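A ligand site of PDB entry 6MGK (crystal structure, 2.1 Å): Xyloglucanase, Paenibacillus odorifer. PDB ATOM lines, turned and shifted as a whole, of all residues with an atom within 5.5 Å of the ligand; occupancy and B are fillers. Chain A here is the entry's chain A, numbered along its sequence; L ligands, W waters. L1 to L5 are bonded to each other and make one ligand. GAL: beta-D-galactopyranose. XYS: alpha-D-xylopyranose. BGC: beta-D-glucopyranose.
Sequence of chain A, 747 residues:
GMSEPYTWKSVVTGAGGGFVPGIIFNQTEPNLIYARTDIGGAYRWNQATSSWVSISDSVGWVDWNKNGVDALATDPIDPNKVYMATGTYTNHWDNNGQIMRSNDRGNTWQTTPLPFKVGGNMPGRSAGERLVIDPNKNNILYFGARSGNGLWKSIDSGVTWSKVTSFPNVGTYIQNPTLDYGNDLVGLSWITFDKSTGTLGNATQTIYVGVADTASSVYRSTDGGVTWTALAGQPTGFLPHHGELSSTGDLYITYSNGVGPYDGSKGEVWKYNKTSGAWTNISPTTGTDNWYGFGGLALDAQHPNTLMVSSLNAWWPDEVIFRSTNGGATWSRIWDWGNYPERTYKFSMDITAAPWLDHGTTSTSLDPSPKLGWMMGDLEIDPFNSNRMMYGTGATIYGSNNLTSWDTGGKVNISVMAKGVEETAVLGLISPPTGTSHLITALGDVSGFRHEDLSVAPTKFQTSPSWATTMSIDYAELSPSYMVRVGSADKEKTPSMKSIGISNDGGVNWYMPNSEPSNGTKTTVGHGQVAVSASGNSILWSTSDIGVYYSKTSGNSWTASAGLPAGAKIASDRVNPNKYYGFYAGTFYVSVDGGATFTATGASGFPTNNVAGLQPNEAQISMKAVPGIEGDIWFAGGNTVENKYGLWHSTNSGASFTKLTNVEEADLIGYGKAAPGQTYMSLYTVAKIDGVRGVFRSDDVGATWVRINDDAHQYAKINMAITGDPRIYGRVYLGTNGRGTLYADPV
An oxygen (O3) of BGC L4 sits at hydrogen-bond distance from the side-chain amide oxygen of Asn 121 (2.6 Å).
The guanidinium group of Arg 125 is in hydrogen-bond range of an oxygen (O2) of BGC L4, 2.9 Å away.
The side-chain carboxylate (OD2) of Asp 445 sits at hydrogen-bond distance from an oxygen (O1) of BGC L4.
The side-chain amide oxygen (OD1) of Asn 737 is in hydrogen-bond range of an oxygen (O2) of BGC L3 (2.7 Å).
OD2 of Asp 38 sits at hydrogen-bond distance from O2 of BGC L4, at 2.7 Å.
The side-chain hydroxyl (OH) of Tyr 181 sits close to an oxygen (O5) of XYS L2.
The side-chain carboxylate of Asp 180 is in hydrogen-bond range of an oxygen (O6) of GAL L1, at 2.6 Å.
The side-chain hydroxyl (OH) of Tyr 262 sits at hydrogen-bond distance from an oxygen (O4) of XYS L2, at 2.7 Å.
The side-chain amide nitrogen of Asn 737 lies close to the side-chain sulfur of Met 720 (3.6 Å).
The guanidinium group (NE) of Arg 125 lies within salt-bridge range of the side-chain carboxylate (OD2) of Asp 38, 3.1 Å away.
OH of Tyr 181 is in hydrogen-bond range of O of Asn 121 (2.6 Å).
N of Gly 444 sits at hydrogen-bond distance from O of Ala 425, at 3.1 Å.
ND2 of Asn 121 is in hydrogen-bond range of OH of Tyr 89.
The backbone carbonyl oxygen (O) of Gly 394 lies within hydrogen-bond range of the backbone NH (N) of Phe 19 (3.3 Å).
OD2 of Asp 38 lies close to OD1 of Asn 121, at 3.4 Å.
N of Asp 445 is in hydrogen-bond range of OG1 of Thr 469 (3.0 Å).
Phe 19 touches the ligand.
CD1 of Ile 39 touches O4 of BGC L4, at 3.5 Å.
Tyr 89 touches the ligand.
CH2 of Trp 93 touches C6 of GAL L1, 3.7 Å away.
Ala 425 touches the ligand.
Gly 444 touches the ligand.
OG1 of Thr 469 touches C2 of XYS L5, at 3.8 Å.
Hydrophobic or aromatic side chains within 4 Å of the ligand: Phe 19, Ile 39, Trp 93, Tyr 181, Tyr 262 and Ala 425.
15 residues have an atom within 4 Å of the ligand: Phe 19, Asp 38, Ile 39, Tyr 89, Trp 93, Asn 121, Arg 125, Asp 180, Tyr 181, Tyr 262, Ala 425, Gly 444, Asp 445, Thr 469 and Asn 737.
Water W4 lies within hydrogen-bond range of an oxygen (O1) of BGC L4 (2.5 Å), the backbone carbonyl oxygen of Gly 394 (2.8 Å) and the side-chain sulfur of Met 375 (3.5 Å).
Water W10 bridges the side-chain hydroxyl of Tyr 89 (2.6 Å) and an oxygen (O3) of BGC L3 (2.8 Å).
Water W8 lies within hydrogen-bond range of OG1 of Thr 469 (2.7 Å) and O2 of XYS L5 (3.2 Å).
Water W5 bridges OD1 of Asp 38 (2.7 Å) and N of Phe 19 (2.9 Å).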
ATOM      1  N   PHE A  19     -27.233  -0.782  -8.319  1.00  0.00           N
ATOM      2  CA  PHE A  19     -28.050   0.412  -8.230  1.00  0.00           C
ATOM      3  C   PHE A  19     -29.086   0.424  -9.360  1.00  0.00           C
ATOM      4  O   PHE A  19     -28.738   0.237 -10.531  1.00  0.00           O
ATOM      5  CB  PHE A  19     -27.164   1.656  -8.318  1.00  0.00           C
ATOM      6  CG  PHE A  19     -27.905   2.967  -8.174  1.00  0.00           C
ATOM      7  CD1 PHE A  19     -29.042   3.065  -7.382  1.00  0.00           C
ATOM      8  CD2 PHE A  19     -27.457   4.094  -8.832  1.00  0.00           C
ATOM      9  CE1 PHE A  19     -29.705   4.267  -7.261  1.00  0.00           C
ATOM     10  CE2 PHE A  19     -28.109   5.300  -8.703  1.00  0.00           C
ATOM     11  CZ  PHE A  19     -29.248   5.390  -7.916  1.00  0.00           C
ATOM     12  N   ASP A  38     -27.273   1.401 -14.203  1.00  0.00           N
ATOM     13  CA  ASP A  38     -26.196   2.281 -14.620  1.00  0.00           C
ATOM     14  C   ASP A  38     -25.085   1.567 -15.378  1.00  0.00           C
ATOM     15  O   ASP A  38     -24.390   2.217 -16.163  1.00  0.00           O
ATOM     16  CB  ASP A  38     -25.595   3.018 -13.415  1.00  0.00           C
ATOM     17  CG  ASP A  38     -25.375   2.116 -12.221  1.00  0.00           C
ATOM     18  OD1 ASP A  38     -25.495   0.876 -12.359  1.00  0.00           O
ATOM     19  OD2 ASP A  38     -25.066   2.654 -11.131  1.00  0.00           O
ATOM     20  N   ILE A  39     -24.906   0.253 -15.205  1.00  0.00           N
ATOM     21  CA  ILE A  39     -23.836  -0.458 -15.882  1.00  0.00           C
ATOM     22  C   ILE A  39     -24.298  -1.808 -16.410  1.00  0.00           C
ATOM     23  O   ILE A  39     -23.508  -2.547 -17.007  1.00  0.00           O
ATOM     24  CB  ILE A  39     -22.609  -0.652 -14.963  1.00  0.00           C
ATOM     25  CG1 ILE A  39     -22.998  -1.451 -13.717  1.00  0.00           C
ATOM     26  CG2 ILE A  39     -21.978   0.688 -14.594  1.00  0.00           C
ATOM     27  CD1 ILE A  39     -21.815  -1.877 -12.880  1.00  0.00           C
ATOM     28  N   TYR A  89     -20.171   6.877 -19.730  1.00  0.00           N
ATOM     29  CA  TYR A  89     -19.458   7.996 -19.144  1.00  0.00           C
ATOM     30  C   TYR A  89     -19.373   9.149 -20.125  1.00  0.00           C
ATOM     31  O   TYR A  89     -19.343   8.954 -21.349  1.00  0.00           O
ATOM     32  CB  TYR A  89     -18.042   7.600 -18.703  1.00  0.00           C
ATOM     33  CG  TYR A  89     -18.030   6.414 -17.768  1.00  0.00           C
ATOM     34  CD1 TYR A  89     -18.507   6.511 -16.475  1.00  0.00           C
ATOM     35  CD2 TYR A  89     -17.546   5.176 -18.204  1.00  0.00           C
ATOM     36  CE1 TYR A  89     -18.496   5.425 -15.622  1.00  0.00           C
ATOM     37  CE2 TYR A  89     -17.534   4.086 -17.365  1.00  0.00           C
ATOM     38  CZ  TYR A  89     -18.007   4.213 -16.078  1.00  0.00           C
ATOM     39  OH  TYR A  89     -17.992   3.131 -15.233  1.00  0.00           O
ATOM     40  N   TRP A  93     -13.418   8.301 -20.283  1.00  0.00           N
ATOM     41  CA  TRP A  93     -13.531   6.859 -20.131  1.00  0.00           C
ATOM     42  C   TRP A  93     -14.422   6.208 -21.180  1.00  0.00           C
ATOM     43  O   TRP A  93     -14.491   4.972 -21.239  1.00  0.00           O
ATOM     44  CB  TRP A  93     -14.101   6.513 -18.751  1.00  0.00           C
ATOM     45  CG  TRP A  93     -13.233   6.882 -17.587  1.00  0.00           C
ATOM     46  CD1 TRP A  93     -11.921   7.275 -17.624  1.00  0.00           C
ATOM     47  CD2 TRP A  93     -13.623   6.893 -16.211  1.00  0.00           C
ATOM     48  NE1 TRP A  93     -11.472   7.532 -16.347  1.00  0.00           N
ATOM     49  CE2 TRP A  93     -12.502   7.302 -15.463  1.00  0.00           C
ATOM     50  CE3 TRP A  93     -14.805   6.593 -15.535  1.00  0.00           C
ATOM     51  CZ2 TRP A  93     -12.525   7.426 -14.075  1.00  0.00           C
ATOM     52  CZ3 TRP A  93     -14.840   6.713 -14.155  1.00  0.00           C
ATOM     53  CH2 TRP A  93     -13.700   7.124 -13.434  1.00  0.00           C
ATOM     54  N   ASN A 121     -23.627   6.072 -16.096  1.00  0.00           N
ATOM     55  CA  ASN A 121     -22.955   5.861 -14.825  1.00  0.00           C
ATOM     56  C   ASN A 121     -22.296   7.139 -14.313  1.00  0.00           C
ATOM     57  O   ASN A 121     -21.255   7.091 -13.658  1.00  0.00           O
ATOM     58  CB  ASN A 121     -21.932   4.734 -14.934  1.00  0.00           C
ATOM     59  CG  ASN A 121     -21.612   4.095 -13.599  1.00  0.00           C
ATOM     60  OD1 ASN A 121     -22.433   4.110 -12.681  1.00  0.00           O
ATOM     61  ND2 ASN A 121     -20.412   3.536 -13.475  1.00  0.00           N
ATOM     62  N   ARG A 125     -27.809  10.308 -12.249  1.00  0.00           N
ATOM     63  CA  ARG A 125     -28.426   9.336 -13.143  1.00  0.00           C
ATOM     64  C   ARG A 125     -29.797   8.874 -12.658  1.00  0.00           C
ATOM     65  O   ARG A 125     -30.547   8.291 -13.456  1.00  0.00           O
ATOM     66  CB  ARG A 125     -27.506   8.132 -13.349  1.00  0.00           C
ATOM     67  CG  ARG A 125     -26.980   7.466 -12.076  1.00  0.00           C
ATOM     68  CD  ARG A 125     -25.877   6.491 -12.460  1.00  0.00           C
ATOM     69  NE  ARG A 125     -25.297   5.773 -11.330  1.00  0.00           N
ATOM     70  CZ  ARG A 125     -24.352   6.263 -10.536  1.00  0.00           C
ATOM     71  NH1 ARG A 125     -23.876   7.486 -10.744  1.00  0.00           N
ATOM     72  NH2 ARG A 125     -23.870   5.531  -9.539  1.00  0.00           N
ATOM     73  N   LEU A 179     -12.145  17.016 -10.117  1.00  0.00           N
ATOM     74  CA  LEU A 179     -11.811  15.619 -10.380  1.00  0.00           C
ATOM     75  C   LEU A 179     -11.905  15.337 -11.870  1.00  0.00           C
ATOM     76  O   LEU A 179     -12.387  16.154 -12.652  1.00  0.00           O
ATOM     77  CB  LEU A 179     -12.752  14.685  -9.596  1.00  0.00           C
ATOM     78  CG  LEU A 179     -12.884  14.923  -8.095  1.00  0.00           C
ATOM     79  CD1 LEU A 179     -13.730  13.827  -7.459  1.00  0.00           C
ATOM     80  CD2 LEU A 179     -11.525  15.004  -7.430  1.00  0.00           C
ATOM     81  N   ASP A 180     -11.427  14.158 -12.262  1.00  0.00           N
ATOM     82  CA  ASP A 180     -11.600  13.696 -13.631  1.00  0.00           C
ATOM     83  C   ASP A 180     -12.892  12.917 -13.822  1.00  0.00           C
ATOM     84  O   ASP A 180     -13.167  12.463 -14.935  1.00  0.00           O
ATOM     85  CB  ASP A 180     -10.393  12.845 -14.067  1.00  0.00           C
ATOM     86  CG  ASP A 180     -10.387  11.465 -13.439  1.00  0.00           C
ATOM     87  OD1 ASP A 180     -10.865  11.321 -12.286  1.00  0.00           O
ATOM     88  OD2 ASP A 180      -9.897  10.515 -14.095  1.00  0.00           O
ATOM     89  N   TYR A 181     -13.680  12.740 -12.759  1.00  0.00           N
ATOM     90  CA  TYR A 181     -14.995  12.112 -12.835  1.00  0.00           C
ATOM     91  C   TYR A 181     -16.044  13.119 -12.380  1.00  0.00           C
ATOM     92  O   TYR A 181     -16.028  13.544 -11.226  1.00  0.00           O
ATOM     93  CB  TYR A 181     -15.059  10.848 -11.972  1.00  0.00           C
ATOM     94  CG  TYR A 181     -16.444  10.241 -11.908  1.00  0.00           C
ATOM     95  CD1 TYR A 181     -16.937   9.475 -12.960  1.00  0.00           C
ATOM     96  CD2 TYR A 181     -17.256  10.445 -10.799  1.00  0.00           C
ATOM     97  CE1 TYR A 181     -18.202   8.926 -12.902  1.00  0.00           C
ATOM     98  CE2 TYR A 181     -18.525   9.891 -10.733  1.00  0.00           C
ATOM     99  CZ  TYR A 181     -18.990   9.134 -11.791  1.00  0.00           C
ATOM    100  OH  TYR A 181     -20.251   8.589 -11.741  1.00  0.00           O
ATOM    101  N   TYR A 262     -25.219   9.767  -4.258  1.00  0.00           N
ATOM    102  CA  TYR A 262     -24.635   9.536  -2.942  1.00  0.00           C
ATOM    103  C   TYR A 262     -24.795  10.702  -1.966  1.00  0.00           C
ATOM    104  O   TYR A 262     -24.734  10.478  -0.762  1.00  0.00           O
ATOM    105  CB  TYR A 262     -23.136   9.224  -3.067  1.00  0.00           C
ATOM    106  CG  TYR A 262     -22.802   8.089  -4.000  1.00  0.00           C
ATOM    107  CD1 TYR A 262     -23.115   6.774  -3.661  1.00  0.00           C
ATOM    108  CD2 TYR A 262     -22.160   8.315  -5.210  1.00  0.00           C
ATOM    109  CE1 TYR A 262     -22.799   5.719  -4.506  1.00  0.00           C
ATOM    110  CE2 TYR A 262     -21.846   7.277  -6.059  1.00  0.00           C
ATOM    111  CZ  TYR A 262     -22.163   5.982  -5.710  1.00  0.00           C
ATOM    112  OH  TYR A 262     -21.853   4.939  -6.551  1.00  0.00           O
ATOM    113  N   MET A 375     -29.760   5.571  -1.419  1.00  0.00           N
ATOM    114  CA  MET A 375     -29.747   6.020  -2.820  1.00  0.00           C
ATOM    115  C   MET A 375     -31.128   5.836  -3.456  1.00  0.00           C
ATOM    116  O   MET A 375     -31.234   5.373  -4.590  1.00  0.00           O
ATOM    117  CB  MET A 375     -28.687   5.268  -3.628  1.00  0.00           C
ATOM    118  CG  MET A 375     -27.260   5.488  -3.163  1.00  0.00           C
ATOM    119  SD  MET A 375     -26.040   4.058  -3.701  1.00  0.00           S
ATOM    120  CE  MET A 375     -25.929   4.458  -5.613  1.00  0.00           C
ATOM    121  N   GLY A 394     -29.417   1.278  -3.819  1.00  0.00           N
ATOM    122  CA  GLY A 394     -28.097   0.943  -4.327  1.00  0.00           C
ATOM    123  C   GLY A 394     -27.832  -0.532  -4.456  1.00  0.00           C
ATOM    124  O   GLY A 394     -26.784  -0.912  -5.002  1.00  0.00           O
ATOM    125  N   ALA A 425     -20.708  -6.264 -10.365  1.00  0.00           N
ATOM    126  CA  ALA A 425     -19.447  -6.300 -11.083  1.00  0.00           C
ATOM    127  C   ALA A 425     -18.586  -7.403 -10.463  1.00  0.00           C
ATOM    128  O   ALA A 425     -18.409  -7.443  -9.245  1.00  0.00           O
ATOM    129  CB  ALA A 425     -18.724  -4.961 -11.009  1.00  0.00           C
ATOM    130  N   LEU A 427     -15.175  -9.224  -9.819  1.00  0.00           N
ATOM    131  CA  LEU A 427     -13.739  -8.976  -9.813  1.00  0.00           C
ATOM    132  C   LEU A 427     -12.916 -10.253  -9.757  1.00  0.00           C
ATOM    133  O   LEU A 427     -11.714 -10.215 -10.083  1.00  0.00           O
ATOM    134  CB  LEU A 427     -13.380  -8.071  -8.635  1.00  0.00           C
ATOM    135  CG  LEU A 427     -14.103  -6.737  -8.809  1.00  0.00           C
ATOM    136  CD1 LEU A 427     -14.441  -6.109  -7.478  1.00  0.00           C
ATOM    137  CD2 LEU A 427     -13.285  -5.794  -9.677  1.00  0.00           C
ATOM    138  N   LEU A 443     -16.958  -9.874  -5.555  1.00  0.00           N
ATOM    139  CA  LEU A 443     -17.863  -8.907  -6.163  1.00  0.00           C
ATOM    140  C   LEU A 443     -17.650  -7.523  -5.564  1.00  0.00           C
ATOM    141  O   LEU A 443     -17.198  -7.380  -4.428  1.00  0.00           O
ATOM    142  CB  LEU A 443     -19.326  -9.299  -5.962  1.00  0.00           C
ATOM    143  CG  LEU A 443     -19.787 -10.685  -6.423  1.00  0.00           C
ATOM    144  CD1 LEU A 443     -21.235 -10.910  -6.004  1.00  0.00           C
ATOM    145  CD2 LEU A 443     -19.639 -10.821  -7.932  1.00  0.00           C
ATOM    146  N   GLY A 444     -18.003  -6.508  -6.355  1.00  0.00           N
ATOM    147  CA  GLY A 444     -18.089  -5.167  -5.820  1.00  0.00           C
ATOM    148  C   GLY A 444     -19.356  -4.973  -5.001  1.00  0.00           C
ATOM    149  O   GLY A 444     -20.371  -5.634  -5.222  1.00  0.00           O
ATOM    150  N   ASP A 445     -19.272  -4.062  -4.035  1.00  0.00           N
ATOM    151  CA  ASP A 445     -20.412  -3.608  -3.240  1.00  0.00           C
ATOM    152  C   ASP A 445     -20.943  -4.653  -2.261  1.00  0.00           C
ATOM    153  O   ASP A 445     -21.223  -4.326  -1.100  1.00  0.00           O
ATOM    154  CB  ASP A 445     -21.547  -3.136  -4.140  1.00  0.00           C
ATOM    155  CG  ASP A 445     -21.235  -1.821  -4.809  1.00  0.00           C
ATOM    156  OD1 ASP A 445     -20.190  -1.215  -4.491  1.00  0.00           O
ATOM    157  OD2 ASP A 445     -22.050  -1.380  -5.639  1.00  0.00           O
ATOM    158  N   THR A 469     -16.206  -4.576  -1.124  1.00  0.00           N
ATOM    159  CA  THR A 469     -15.694  -5.050  -2.404  1.00  0.00           C
ATOM    160  C   THR A 469     -14.516  -5.991  -2.185  1.00  0.00           C
ATOM    161  O   THR A 469     -13.493  -5.596  -1.622  1.00  0.00           O
ATOM    162  CB  THR A 469     -15.268  -3.860  -3.277  1.00  0.00           C
ATOM    163  OG1 THR A 469     -16.432  -3.129  -3.685  1.00  0.00           O
ATOM    164  CG2 THR A 469     -14.512  -4.336  -4.496  1.00  0.00           C
ATOM    165  N   MET A 471     -11.600  -7.630  -4.041  1.00  0.00           N
ATOM    166  CA  MET A 471     -10.858  -7.394  -5.270  1.00  0.00           C
ATOM    167  C   MET A 471     -10.202  -8.622  -5.840  1.00  0.00           C
ATOM    168  O   MET A 471      -9.960  -8.652  -7.061  1.00  0.00           O
ATOM    169  CB  MET A 471      -9.778  -6.347  -4.993  1.00  0.00           C
ATOM    170  CG  MET A 471      -9.205  -5.813  -6.300  1.00  0.00           C
ATOM    171  SD  MET A 471     -10.563  -4.717  -7.216  1.00  0.00           S
ATOM    172  CE  MET A 471     -10.996  -3.506  -5.720  1.00  0.00           C
ATOM    173  N   PRO A 616     -10.727   2.777 -19.114  1.00  0.00           N
ATOM    174  CA  PRO A 616     -10.443   1.927 -17.946  1.00  0.00           C
ATOM    175  C   PRO A 616     -10.771   0.442 -18.118  1.00  0.00           C
ATOM    176  O   PRO A 616     -10.102  -0.393 -17.491  1.00  0.00           O
ATOM    177  CB  PRO A 616     -11.323   2.557 -16.853  1.00  0.00           C
ATOM    178  CG  PRO A 616     -11.394   3.974 -17.227  1.00  0.00           C
ATOM    179  CD  PRO A 616     -11.422   4.017 -18.735  1.00  0.00           C
ATOM    180  N   ASN A 617     -11.757   0.088 -18.943  1.00  0.00           N
ATOM    181  CA  ASN A 617     -12.143  -1.303 -19.115  1.00  0.00           C
ATOM    182  C   ASN A 617     -11.798  -1.846 -20.495  1.00  0.00           C
ATOM    183  O   ASN A 617     -12.407  -2.818 -20.942  1.00  0.00           O
ATOM    184  CB  ASN A 617     -13.642  -1.471 -18.840  1.00  0.00           C
ATOM    185  CG  ASN A 617     -14.501  -0.554 -19.694  1.00  0.00           C
ATOM    186  OD1 ASN A 617     -14.303  -0.430 -20.899  1.00  0.00           O
ATOM    187  ND2 ASN A 617     -15.487   0.088 -19.078  1.00  0.00           N
ATOM    188  N   MET A 720     -13.690  -9.349 -17.165  1.00  0.00           N
ATOM    189  CA  MET A 720     -13.627  -9.322 -15.714  1.00  0.00           C
ATOM    190  C   MET A 720     -13.048 -10.609 -15.130  1.00  0.00           C
ATOM    191  O   MET A 720     -12.044 -10.563 -14.413  1.00  0.00           O
ATOM    192  CB  MET A 720     -15.022  -9.065 -15.139  1.00  0.00           C
ATOM    193  CG  MET A 720     -15.616  -7.727 -15.561  1.00  0.00           C
ATOM    194  SD  MET A 720     -14.536  -6.209 -14.972  1.00  0.00           S
ATOM    195  CE  MET A 720     -15.318  -5.946 -13.208  1.00  0.00           C
ATOM    196  N   ASN A 737     -19.332  -6.948 -15.931  1.00  0.00           N
ATOM    197  CA  ASN A 737     -19.275  -5.650 -15.272  1.00  0.00           C
ATOM    198  C   ASN A 737     -20.679  -5.043 -15.345  1.00  0.00           C
ATOM    199  O   ASN A 737     -20.952  -4.150 -16.141  1.00  0.00           O
ATOM    200  CB  ASN A 737     -18.224  -4.748 -15.918  1.00  0.00           C
ATOM    201  CG  ASN A 737     -17.838  -3.572 -15.035  1.00  0.00           C
ATOM    202  OD1 ASN A 737     -18.673  -3.013 -14.314  1.00  0.00           O
ATOM    203  ND2 ASN A 737     -16.565  -3.192 -15.074  1.00  0.00           N
HETATM  204  C1  GAL L   1     -15.327   7.230  -8.144  1.00  0.00           C
HETATM  205  C2  GAL L   1     -14.616   7.068  -6.800  1.00  0.00           C
HETATM  206  C3  GAL L   1     -13.544   8.069  -6.580  1.00  0.00           C
HETATM  207  C4  GAL L   1     -12.601   8.167  -7.736  1.00  0.00           C
HETATM  208  C5  GAL L   1     -13.349   8.409  -9.053  1.00  0.00           C
HETATM  209  C6  GAL L   1     -12.370   8.429 -10.186  1.00  0.00           C
HETATM  210  O2  GAL L   1     -15.599   7.188  -5.752  1.00  0.00           O
HETATM  211  O3  GAL L   1     -12.803   7.696  -5.394  1.00  0.00           O
HETATM  212  O4  GAL L   1     -11.861   6.944  -7.843  1.00  0.00           O
HETATM  213  O5  GAL L   1     -14.363   7.374  -9.301  1.00  0.00           O
HETATM  214  O6  GAL L   1     -12.061   9.764 -10.515  1.00  0.00           O
HETATM  215  C1  XYS L   2     -17.019   5.930 -10.576  1.00  0.00           C
HETATM  216  C2  XYS L   2     -17.298   6.497  -9.186  1.00  0.00           C
HETATM  217  C3  XYS L   2     -18.555   5.934  -8.626  1.00  0.00           C
HETATM  218  C4  XYS L   2     -19.716   6.152  -9.535  1.00  0.00           C
HETATM  219  C5  XYS L   2     -19.445   5.623 -10.956  1.00  0.00           C
HETATM  220  O2  XYS L   2     -16.213   6.118  -8.322  1.00  0.00           O
HETATM  221  O3  XYS L   2     -18.825   6.557  -7.351  1.00  0.00           O
HETATM  222  O4  XYS L   2     -20.852   5.465  -9.010  1.00  0.00           O
HETATM  223  O5  XYS L   2     -18.168   6.113 -11.512  1.00  0.00           O
HETATM  224  C2  BGC L   3     -18.040   0.114 -12.524  1.00  0.00           C
HETATM  225  C3  BGC L   3     -16.567   0.307 -12.683  1.00  0.00           C
HETATM  226  C4  BGC L   3     -16.184   1.749 -12.736  1.00  0.00           C
HETATM  227  C5  BGC L   3     -16.780   2.523 -11.552  1.00  0.00           C
HETATM  228  C6  BGC L   3     -16.405   3.968 -11.658  1.00  0.00           C
HETATM  229  C1  BGC L   3     -18.618   0.939 -11.365  1.00  0.00           C
HETATM  230  O2  BGC L   3     -18.294  -1.286 -12.267  1.00  0.00           O
HETATM  231  O3  BGC L   3     -16.155  -0.334 -13.921  1.00  0.00           O
HETATM  232  O4  BGC L   3     -14.761   1.867 -12.686  1.00  0.00           O
HETATM  233  O5  BGC L   3     -18.240   2.391 -11.515  1.00  0.00           O
HETATM  234  O6  BGC L   3     -16.655   4.552 -10.407  1.00  0.00           O
HETATM  235  C2  BGC L   4     -22.350   2.066  -8.656  1.00  0.00           C
HETATM  236  C3  BGC L   4     -21.716   1.849  -9.989  1.00  0.00           C
HETATM  237  C4  BGC L   4     -20.513   0.947  -9.937  1.00  0.00           C
HETATM  238  C5  BGC L   4     -20.893  -0.389  -9.265  1.00  0.00           C
HETATM  239  C6  BGC L   4     -19.747  -1.353  -9.140  1.00  0.00           C
HETATM  240  C1  BGC L   4     -22.587   0.769  -7.887  1.00  0.00           C
HETATM  241  O1  BGC L   4     -22.886   1.073  -6.598  1.00  0.00           O
HETATM  242  O2  BGC L   4     -23.614   2.718  -8.846  1.00  0.00           O
HETATM  243  O3  BGC L   4     -21.331   3.152 -10.513  1.00  0.00           O
HETATM  244  O4  BGC L   4     -20.052   0.722 -11.275  1.00  0.00           O
HETATM  245  O5  BGC L   4     -21.399  -0.128  -7.904  1.00  0.00           O
HETATM  246  O6  BGC L   4     -18.709  -0.757  -8.389  1.00  0.00           O
HETATM  247  C1  XYS L   5     -18.033  -1.761  -7.603  1.00  0.00           C
HETATM  248  C2  XYS L   5     -16.863  -1.106  -6.864  1.00  0.00           C
HETATM  249  C3  XYS L   5     -15.834  -0.658  -7.836  1.00  0.00           C
HETATM  250  C4  XYS L   5     -15.305  -1.812  -8.630  1.00  0.00           C
HETATM  251  C5  XYS L   5     -16.427  -2.605  -9.323  1.00  0.00           C
HETATM  252  O2  XYS L   5     -17.329   0.018  -6.106  1.00  0.00           O
HETATM  253  O3  XYS L   5     -14.738  -0.023  -7.108  1.00  0.00           O
HETATM  254  O4  XYS L   5     -14.415  -1.315  -9.631  1.00  0.00           O
HETATM  255  O5  XYS L   5     -17.562  -2.930  -8.423  1.00  0.00           O
HETATM  256  O   HOH W   1     -13.890   2.800 -14.987  1.00  0.00           O
HETATM  257  O   HOH W   2     -13.402   1.646 -10.097  1.00  0.00           O
HETATM  258  O   HOH W   3     -18.932   9.334  -6.889  1.00  0.00           O
HETATM  259  O   HOH W   4     -24.901   1.108  -5.090  1.00  0.00           O
HETATM  260  O   HOH W   5     -24.934  -0.330 -10.017  1.00  0.00           O
HETATM  261  O   HOH W   6     -18.125   5.385  -5.006  1.00  0.00           O
HETATM  262  O   HOH W   7     -15.415   3.223  -7.980  1.00  0.00           O
HETATM  263  O   HOH W   8     -15.758  -0.555  -3.347  1.00  0.00           O
HETATM  264  O   HOH W   9     -12.337   3.535 -12.893  1.00  0.00           O
HETATM  265  O   HOH W  10     -17.387   0.812 -16.173  1.00  0.00           O
